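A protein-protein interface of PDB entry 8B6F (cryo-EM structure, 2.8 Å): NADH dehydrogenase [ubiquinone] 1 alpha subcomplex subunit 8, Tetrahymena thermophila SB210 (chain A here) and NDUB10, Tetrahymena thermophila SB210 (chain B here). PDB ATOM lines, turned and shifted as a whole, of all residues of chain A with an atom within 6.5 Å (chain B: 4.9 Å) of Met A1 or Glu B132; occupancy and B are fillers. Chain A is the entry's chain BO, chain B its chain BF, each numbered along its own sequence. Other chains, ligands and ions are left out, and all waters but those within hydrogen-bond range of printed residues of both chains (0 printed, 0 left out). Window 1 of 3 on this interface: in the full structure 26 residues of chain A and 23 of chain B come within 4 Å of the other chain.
The side-chain carboxylate (OD1) of Asp B52 lies within salt-bridge range of the guanidinium group (NE) of Arg A118.
The backbone carbonyl oxygen (O) of Phe A18 sits at hydrogen-bond distance from the side-chain amide nitrogen (ND2) of Asn B129 (3.0 Å).
The backbone carbonyl oxygen (O) of Met A1 sits close to the side-chain carboxylate (OE1) of Glu B132, at 3.2 Å.
NZ of Lys B59 lies within salt-bridge range of OE2 of Glu B132 (2.6 Å).
O of Glu B132 sits at hydrogen-bond distance from OG1 of Thr B136, 2.9 Å away.
The backbone carbonyl oxygen (O) of Phe A2 lies within hydrogen-bond range of the backbone NH (N) of Phe A18, at 3.0 Å.
The guanidinium group (NE) of Arg A117 is in salt-bridge range of the side-chain carboxylate (OD2) of Asp A121 (3.3 Å).
Among the printed residues, merely in contact across the chains: Met A1 with Leu B48, Phe A2 with Leu B48, Phe A2 with Asn B129, Leu A3 with Asn B129, Leu A3 with Glu B132, Val A15 with Glu B133, Val A15 with Thr B136 and Arg A117 with Leu B48.
Of chain B, only Leu B48 and Glu B132 come within 4 Å of Met A1.
Of the printed residues of chain B, Phe A2 touches Leu B48 and Asn B129.
Of the printed residues of chain B, Leu A3 touches Asn B129 and Glu B132.
Of the printed residues of chain B, Val A15 touches Glu B133 and Thr B136.
Of the printed residues of chain B, Arg A117 touches Leu B48 (3.8 Å).
Gln A122 touches none of the printed residues of chain B.
Tyr B130 touches none of the printed residues of chain A.
Glu B132 touches just these residues of chain A: Met A1 (3.2 Å) and Leu A3 (3.2 Å).
The nearest residue of chain B that does not touch Met A1 is Asn B129 (4.2 Å).
Of the 11 printed residues of chain A, 7 touch a printed residue of chain B.
Printed residues of chain A that touch a printed residue of chain B: Met A1, Phe A2, Leu A3, Val A15, Phe A18, Arg A117 and Arg A118.
Along chain A the printed residues that touch a printed residue of chain B span positions 1 to 118.
Of the 12 printed residues of chain B, 6 touch a printed residue of chain A.
Among the printed residues, Asp or Glu carboxylates within 4 Å of a Lys or Arg side-chain nitrogen of the other chain: Arg A118 with Asp B52 (3.2 Å).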
ATOM      1  N   MET A   1      14.697  10.914  -3.308  1.00  0.00           N
ATOM      2  CA  MET A   1      15.386  10.086  -2.278  1.00  0.00           C
ATOM      3  C   MET A   1      15.850  10.973  -1.128  1.00  0.00           C
ATOM      4  O   MET A   1      16.510  11.988  -1.346  1.00  0.00           O
ATOM      5  CB  MET A   1      16.572   9.341  -2.896  1.00  0.00           C
ATOM      6  CG  MET A   1      16.985   8.089  -2.137  1.00  0.00           C
ATOM      7  SD  MET A   1      18.315   7.189  -2.962  1.00  0.00           S
ATOM      8  CE  MET A   1      18.479   5.756  -1.900  1.00  0.00           C
ATOM      9  N   PHE A   2      15.493  10.586   0.096  1.00  0.00           N
ATOM     10  CA  PHE A   2      15.795  11.374   1.291  1.00  0.00           C
ATOM     11  C   PHE A   2      15.079  12.719   1.269  1.00  0.00           C
ATOM     12  O   PHE A   2      15.546  13.692   1.864  1.00  0.00           O
ATOM     13  CB  PHE A   2      17.305  11.580   1.455  1.00  0.00           C
ATOM     14  CG  PHE A   2      18.098  10.310   1.389  1.00  0.00           C
ATOM     15  CD1 PHE A   2      18.041   9.390   2.422  1.00  0.00           C
ATOM     16  CD2 PHE A   2      18.907  10.040   0.299  1.00  0.00           C
ATOM     17  CE1 PHE A   2      18.773   8.221   2.365  1.00  0.00           C
ATOM     18  CE2 PHE A   2      19.640   8.871   0.237  1.00  0.00           C
ATOM     19  CZ  PHE A   2      19.572   7.961   1.272  1.00  0.00           C
ATOM     20  N   LEU A   3      13.943  12.783   0.580  1.00  0.00           N
ATOM     21  CA  LEU A   3      13.122  13.984   0.501  1.00  0.00           C
ATOM     22  C   LEU A   3      11.745  13.687   1.077  1.00  0.00           C
ATOM     23  O   LEU A   3      11.130  12.674   0.732  1.00  0.00           O
ATOM     24  CB  LEU A   3      12.995  14.472  -0.945  1.00  0.00           C
ATOM     25  CG  LEU A   3      14.010  15.524  -1.398  1.00  0.00           C
ATOM     26  CD1 LEU A   3      15.431  15.058  -1.163  1.00  0.00           C
ATOM     27  CD2 LEU A   3      13.805  15.851  -2.862  1.00  0.00           C
ATOM     28  N   VAL A  15       8.613  19.347  -1.663  1.00  0.00           N
ATOM     29  CA  VAL A  15       9.423  18.386  -0.926  1.00  0.00           C
ATOM     30  C   VAL A  15      10.503  19.128  -0.155  1.00  0.00           C
ATOM     31  O   VAL A  15      11.109  20.076  -0.666  1.00  0.00           O
ATOM     32  CB  VAL A  15      10.047  17.340  -1.870  1.00  0.00           C
ATOM     33  CG1 VAL A  15       8.969  16.461  -2.476  1.00  0.00           C
ATOM     34  CG2 VAL A  15      10.846  18.031  -2.963  1.00  0.00           C
ATOM     35  N   PHE A  18      15.799  15.772   4.069  1.00  0.00           N
ATOM     36  CA  PHE A  18      16.266  15.394   5.393  1.00  0.00           C
ATOM     37  C   PHE A  18      17.501  14.519   5.242  1.00  0.00           C
ATOM     38  O   PHE A  18      17.725  13.906   4.195  1.00  0.00           O
ATOM     39  CB  PHE A  18      15.184  14.656   6.194  1.00  0.00           C
ATOM     40  CG  PHE A  18      14.879  13.280   5.677  1.00  0.00           C
ATOM     41  CD1 PHE A  18      13.921  13.093   4.698  1.00  0.00           C
ATOM     42  CD2 PHE A  18      15.543  12.174   6.180  1.00  0.00           C
ATOM     43  CE1 PHE A  18      13.637  11.828   4.223  1.00  0.00           C
ATOM     44  CE2 PHE A  18      15.262  10.908   5.710  1.00  0.00           C
ATOM     45  CZ  PHE A  18      14.308  10.735   4.730  1.00  0.00           C
ATOM     46  N   ARG A 117      17.036  -1.368  -5.980  1.00  0.00           N
ATOM     47  CA  ARG A 117      17.771  -1.323  -4.721  1.00  0.00           C
ATOM     48  C   ARG A 117      17.385  -0.103  -3.901  1.00  0.00           C
ATOM     49  O   ARG A 117      17.432  -0.143  -2.666  1.00  0.00           O
ATOM     50  CB  ARG A 117      19.278  -1.321  -4.973  1.00  0.00           C
ATOM     51  CG  ARG A 117      20.079  -0.790  -3.788  1.00  0.00           C
ATOM     52  CD  ARG A 117      21.557  -1.098  -3.906  1.00  0.00           C
ATOM     53  NE  ARG A 117      22.312  -0.515  -2.802  1.00  0.00           N
ATOM     54  CZ  ARG A 117      23.590  -0.763  -2.549  1.00  0.00           C
ATOM     55  NH1 ARG A 117      24.293  -1.599  -3.295  1.00  0.00           N
ATOM     56  NH2 ARG A 117      24.179  -0.153  -1.525  1.00  0.00           N
ATOM     57  N   ARG A 118      16.998   0.985  -4.565  1.00  0.00           N
ATOM     58  CA  ARG A 118      16.546   2.166  -3.841  1.00  0.00           C
ATOM     59  C   ARG A 118      15.341   1.838  -2.974  1.00  0.00           C
ATOM     60  O   ARG A 118      15.275   2.243  -1.808  1.00  0.00           O
ATOM     61  CB  ARG A 118      16.212   3.285  -4.827  1.00  0.00           C
ATOM     62  CG  ARG A 118      17.388   3.694  -5.699  1.00  0.00           C
ATOM     63  CD  ARG A 118      16.955   4.595  -6.840  1.00  0.00           C
ATOM     64  NE  ARG A 118      18.040   4.809  -7.788  1.00  0.00           N
ATOM     65  CZ  ARG A 118      17.917   5.455  -8.938  1.00  0.00           C
ATOM     66  NH1 ARG A 118      16.763   5.974  -9.321  1.00  0.00           N
ATOM     67  NH2 ARG A 118      18.979   5.579  -9.729  1.00  0.00           N
ATOM     68  N   PHE A 119      14.375   1.103  -3.526  1.00  0.00           N
ATOM     69  CA  PHE A 119      13.185   0.762  -2.759  1.00  0.00           C
ATOM     70  C   PHE A 119      13.489  -0.270  -1.682  1.00  0.00           C
ATOM     71  O   PHE A 119      12.922  -0.210  -0.585  1.00  0.00           O
ATOM     72  CB  PHE A 119      12.091   0.264  -3.699  1.00  0.00           C
ATOM     73  CG  PHE A 119      11.682   1.278  -4.723  1.00  0.00           C
ATOM     74  CD1 PHE A 119      10.884   2.351  -4.368  1.00  0.00           C
ATOM     75  CD2 PHE A 119      12.100   1.165  -6.037  1.00  0.00           C
ATOM     76  CE1 PHE A 119      10.507   3.291  -5.303  1.00  0.00           C
ATOM     77  CE2 PHE A 119      11.726   2.101  -6.979  1.00  0.00           C
ATOM     78  CZ  PHE A 119      10.928   3.166  -6.611  1.00  0.00           C
ATOM     79  N   ASP A 121      16.382  -0.616  -0.076  1.00  0.00           N
ATOM     80  CA  ASP A 121      17.024   0.166   0.973  1.00  0.00           C
ATOM     81  C   ASP A 121      16.022   1.047   1.700  1.00  0.00           C
ATOM     82  O   ASP A 121      16.164   1.285   2.904  1.00  0.00           O
ATOM     83  CB  ASP A 121      18.142   1.024   0.384  1.00  0.00           C
ATOM     84  CG  ASP A 121      19.314   0.198  -0.109  1.00  0.00           C
ATOM     85  OD1 ASP A 121      19.249  -1.044  -0.009  1.00  0.00           O
ATOM     86  OD2 ASP A 121      20.303   0.794  -0.588  1.00  0.00           O
ATOM     87  N   GLN A 122      14.993   1.521   0.998  1.00  0.00           N
ATOM     88  CA  GLN A 122      13.950   2.290   1.663  1.00  0.00           C
ATOM     89  C   GLN A 122      13.197   1.428   2.667  1.00  0.00           C
ATOM     90  O   GLN A 122      12.852   1.894   3.758  1.00  0.00           O
ATOM     91  CB  GLN A 122      12.993   2.883   0.630  1.00  0.00           C
ATOM     92  CG  GLN A 122      11.870   3.718   1.229  1.00  0.00           C
ATOM     93  CD  GLN A 122      12.383   4.847   2.105  1.00  0.00           C
ATOM     94  OE1 GLN A 122      13.524   5.286   1.967  1.00  0.00           O
ATOM     95  NE2 GLN A 122      11.539   5.324   3.012  1.00  0.00           N
ATOM     96  N   ARG A 125      15.497   1.144   5.617  1.00  0.00           N
ATOM     97  CA  ARG A 125      15.543   2.411   6.339  1.00  0.00           C
ATOM     98  C   ARG A 125      14.261   2.652   7.124  1.00  0.00           C
ATOM     99  O   ARG A 125      14.305   3.168   8.246  1.00  0.00           O
ATOM    100  CB  ARG A 125      15.788   3.559   5.360  1.00  0.00           C
ATOM    101  CG  ARG A 125      17.148   3.522   4.693  1.00  0.00           C
ATOM    102  CD  ARG A 125      17.189   4.444   3.489  1.00  0.00           C
ATOM    103  NE  ARG A 125      18.412   4.275   2.715  1.00  0.00           N
ATOM    104  CZ  ARG A 125      19.576   4.833   3.016  1.00  0.00           C
ATOM    105  NH1 ARG A 125      19.725   5.588   4.091  1.00  0.00           N
ATOM    106  NH2 ARG A 125      20.619   4.628   2.218  1.00  0.00           N
ATOM    107  N   LEU B  48      24.874   4.357  -0.103  1.00  0.00           N
ATOM    108  CA  LEU B  48      24.400   4.366  -1.477  1.00  0.00           C
ATOM    109  C   LEU B  48      25.219   3.416  -2.342  1.00  0.00           C
ATOM    110  O   LEU B  48      26.380   3.120  -2.051  1.00  0.00           O
ATOM    111  CB  LEU B  48      24.475   5.779  -2.052  1.00  0.00           C
ATOM    112  CG  LEU B  48      23.757   6.868  -1.253  1.00  0.00           C
ATOM    113  CD1 LEU B  48      23.966   8.226  -1.898  1.00  0.00           C
ATOM    114  CD2 LEU B  48      22.277   6.560  -1.123  1.00  0.00           C
ATOM    115  N   ASP B  52      24.210   5.309  -7.364  1.00  0.00           N
ATOM    116  CA  ASP B  52      23.601   6.322  -6.510  1.00  0.00           C
ATOM    117  C   ASP B  52      24.635   7.310  -5.991  1.00  0.00           C
ATOM    118  O   ASP B  52      24.362   8.512  -5.899  1.00  0.00           O
ATOM    119  CB  ASP B  52      22.860   5.657  -5.352  1.00  0.00           C
ATOM    120  CG  ASP B  52      21.586   4.970  -5.797  1.00  0.00           C
ATOM    121  OD1 ASP B  52      20.996   5.411  -6.804  1.00  0.00           O
ATOM    122  OD2 ASP B  52      21.172   3.994  -5.139  1.00  0.00           O
ATOM    123  N   LYS B  59      25.572  15.714  -8.021  1.00  0.00           N
ATOM    124  CA  LYS B  59      24.682  16.698  -7.415  1.00  0.00           C
ATOM    125  C   LYS B  59      25.434  17.584  -6.431  1.00  0.00           C
ATOM    126  O   LYS B  59      25.152  18.783  -6.328  1.00  0.00           O
ATOM    127  CB  LYS B  59      23.515  15.992  -6.727  1.00  0.00           C
ATOM    128  CG  LYS B  59      22.532  15.356  -7.696  1.00  0.00           C
ATOM    129  CD  LYS B  59      21.490  14.528  -6.968  1.00  0.00           C
ATOM    130  CE  LYS B  59      20.546  13.853  -7.950  1.00  0.00           C
ATOM    131  NZ  LYS B  59      19.592  12.934  -7.265  1.00  0.00           N
ATOM    132  N   VAL B 128      23.099  18.271  -1.363  1.00  0.00           N
ATOM    133  CA  VAL B 128      22.485  17.424  -2.382  1.00  0.00           C
ATOM    134  C   VAL B 128      20.967  17.481  -2.279  1.00  0.00           C
ATOM    135  O   VAL B 128      20.260  17.476  -3.294  1.00  0.00           O
ATOM    136  CB  VAL B 128      23.016  15.984  -2.264  1.00  0.00           C
ATOM    137  CG1 VAL B 128      22.198  15.024  -3.118  1.00  0.00           C
ATOM    138  CG2 VAL B 128      24.477  15.936  -2.664  1.00  0.00           C
ATOM    139  N   ASN B 129      20.440  17.531  -1.055  1.00  0.00           N
ATOM    140  CA  ASN B 129      18.996  17.642  -0.884  1.00  0.00           C
ATOM    141  C   ASN B 129      18.479  18.964  -1.428  1.00  0.00           C
ATOM    142  O   ASN B 129      17.406  19.016  -2.039  1.00  0.00           O
ATOM    143  CB  ASN B 129      18.627  17.499   0.593  1.00  0.00           C
ATOM    144  CG  ASN B 129      18.766  16.079   1.094  1.00  0.00           C
ATOM    145  OD1 ASN B 129      18.711  15.127   0.318  1.00  0.00           O
ATOM    146  ND2 ASN B 129      18.942  15.929   2.401  1.00  0.00           N
ATOM    147  N   TYR B 130      19.228  20.046  -1.214  1.00  0.00           N
ATOM    148  CA  TYR B 130      18.834  21.334  -1.767  1.00  0.00           C
ATOM    149  C   TYR B 130      18.819  21.293  -3.290  1.00  0.00           C
ATOM    150  O   TYR B 130      17.885  21.796  -3.924  1.00  0.00           O
ATOM    151  CB  TYR B 130      19.783  22.413  -1.253  1.00  0.00           C
ATOM    152  CG  TYR B 130      19.369  23.824  -1.578  1.00  0.00           C
ATOM    153  CD1 TYR B 130      18.215  24.362  -1.025  1.00  0.00           C
ATOM    154  CD2 TYR B 130      20.147  24.631  -2.393  1.00  0.00           C
ATOM    155  CE1 TYR B 130      17.831  25.651  -1.297  1.00  0.00           C
ATOM    156  CE2 TYR B 130      19.771  25.926  -2.672  1.00  0.00           C
ATOM    157  CZ  TYR B 130      18.614  26.430  -2.113  1.00  0.00           C
ATOM    158  OH  TYR B 130      18.234  27.717  -2.383  1.00  0.00           O
ATOM    159  N   VAL B 131      19.849  20.701  -3.897  1.00  0.00           N
ATOM    160  CA  VAL B 131      19.891  20.578  -5.351  1.00  0.00           C
ATOM    161  C   VAL B 131      18.714  19.747  -5.846  1.00  0.00           C
ATOM    162  O   VAL B 131      18.084  20.075  -6.858  1.00  0.00           O
ATOM    163  CB  VAL B 131      21.238  19.980  -5.798  1.00  0.00           C
ATOM    164  CG1 VAL B 131      21.237  19.697  -7.294  1.00  0.00           C
ATOM    165  CG2 VAL B 131      22.375  20.919  -5.446  1.00  0.00           C
ATOM    166  N   GLU B 132      18.396  18.662  -5.137  1.00  0.00           N
ATOM    167  CA  GLU B 132      17.278  17.812  -5.531  1.00  0.00           C
ATOM    168  C   GLU B 132      15.942  18.523  -5.369  1.00  0.00           C
ATOM    169  O   GLU B 132      15.024  18.296  -6.164  1.00  0.00           O
ATOM    170  CB  GLU B 132      17.293  16.515  -4.723  1.00  0.00           C
ATOM    171  CG  GLU B 132      18.411  15.564  -5.119  1.00  0.00           C
ATOM    172  CD  GLU B 132      18.415  14.289  -4.299  1.00  0.00           C
ATOM    173  OE1 GLU B 132      17.716  14.239  -3.265  1.00  0.00           O
ATOM    174  OE2 GLU B 132      19.116  13.332  -4.691  1.00  0.00           O
ATOM    175  N   GLU B 133      15.804  19.373  -4.350  1.00  0.00           N
ATOM    176  CA  GLU B 133      14.584  20.164  -4.223  1.00  0.00           C
ATOM    177  C   GLU B 133      14.417  21.100  -5.412  1.00  0.00           C
ATOM    178  O   GLU B 133      13.317  21.227  -5.962  1.00  0.00           O
ATOM    179  CB  GLU B 133      14.605  20.961  -2.919  1.00  0.00           C
ATOM    180  CG  GLU B 133      14.469  20.110  -1.672  1.00  0.00           C
ATOM    181  CD  GLU B 133      14.736  20.898  -0.404  1.00  0.00           C
ATOM    182  OE1 GLU B 133      14.781  22.144  -0.478  1.00  0.00           O
ATOM    183  OE2 GLU B 133      14.905  20.276   0.664  1.00  0.00           O
ATOM    184  N   LYS B 134      15.493  21.774  -5.817  1.00  0.00           N
ATOM    185  CA  LYS B 134      15.418  22.637  -6.990  1.00  0.00           C
ATOM    186  C   LYS B 134      15.087  21.829  -8.238  1.00  0.00           C
ATOM    187  O   LYS B 134      14.297  22.268  -9.081  1.00  0.00           O
ATOM    188  CB  LYS B 134      16.734  23.395  -7.166  1.00  0.00           C
ATOM    189  CG  LYS B 134      17.078  24.312  -6.000  1.00  0.00           C
ATOM    190  CD  LYS B 134      16.058  25.430  -5.840  1.00  0.00           C
ATOM    191  CE  LYS B 134      16.386  26.306  -4.643  1.00  0.00           C
ATOM    192  NZ  LYS B 134      15.376  27.384  -4.458  1.00  0.00           N
ATOM    193  N   GLN B 135      15.690  20.645  -8.378  1.00  0.00           N
ATOM    194  CA  GLN B 135      15.397  19.795  -9.528  1.00  0.00           C
ATOM    195  C   GLN B 135      13.935  19.373  -9.539  1.00  0.00           C
ATOM    196  O   GLN B 135      13.293  19.356 -10.596  1.00  0.00           O
ATOM    197  CB  GLN B 135      16.297  18.562  -9.525  1.00  0.00           C
ATOM    198  CG  GLN B 135      17.715  18.823  -9.985  1.00  0.00           C
ATOM    199  CD  GLN B 135      18.481  17.538 -10.215  1.00  0.00           C
ATOM    200  OE1 GLN B 135      19.157  17.037  -9.321  1.00  0.00           O
ATOM    201  NE2 GLN B 135      18.374  16.995 -11.422  1.00  0.00           N
ATOM    202  N   THR B 136      13.389  19.026  -8.373  1.00  0.00           N
ATOM    203  CA  THR B 136      11.982  18.654  -8.306  1.00  0.00           C
ATOM    204  C   THR B 136      11.093  19.818  -8.712  1.00  0.00           C
ATOM    205  O   THR B 136      10.140  19.642  -9.480  1.00  0.00           O
ATOM    206  CB  THR B 136      11.628  18.185  -6.895  1.00  0.00           C
ATOM    207  OG1 THR B 136      12.441  17.061  -6.541  1.00  0.00           O
ATOM    208  CG2 THR B 136      10.161  17.787  -6.808  1.00  0.00           C
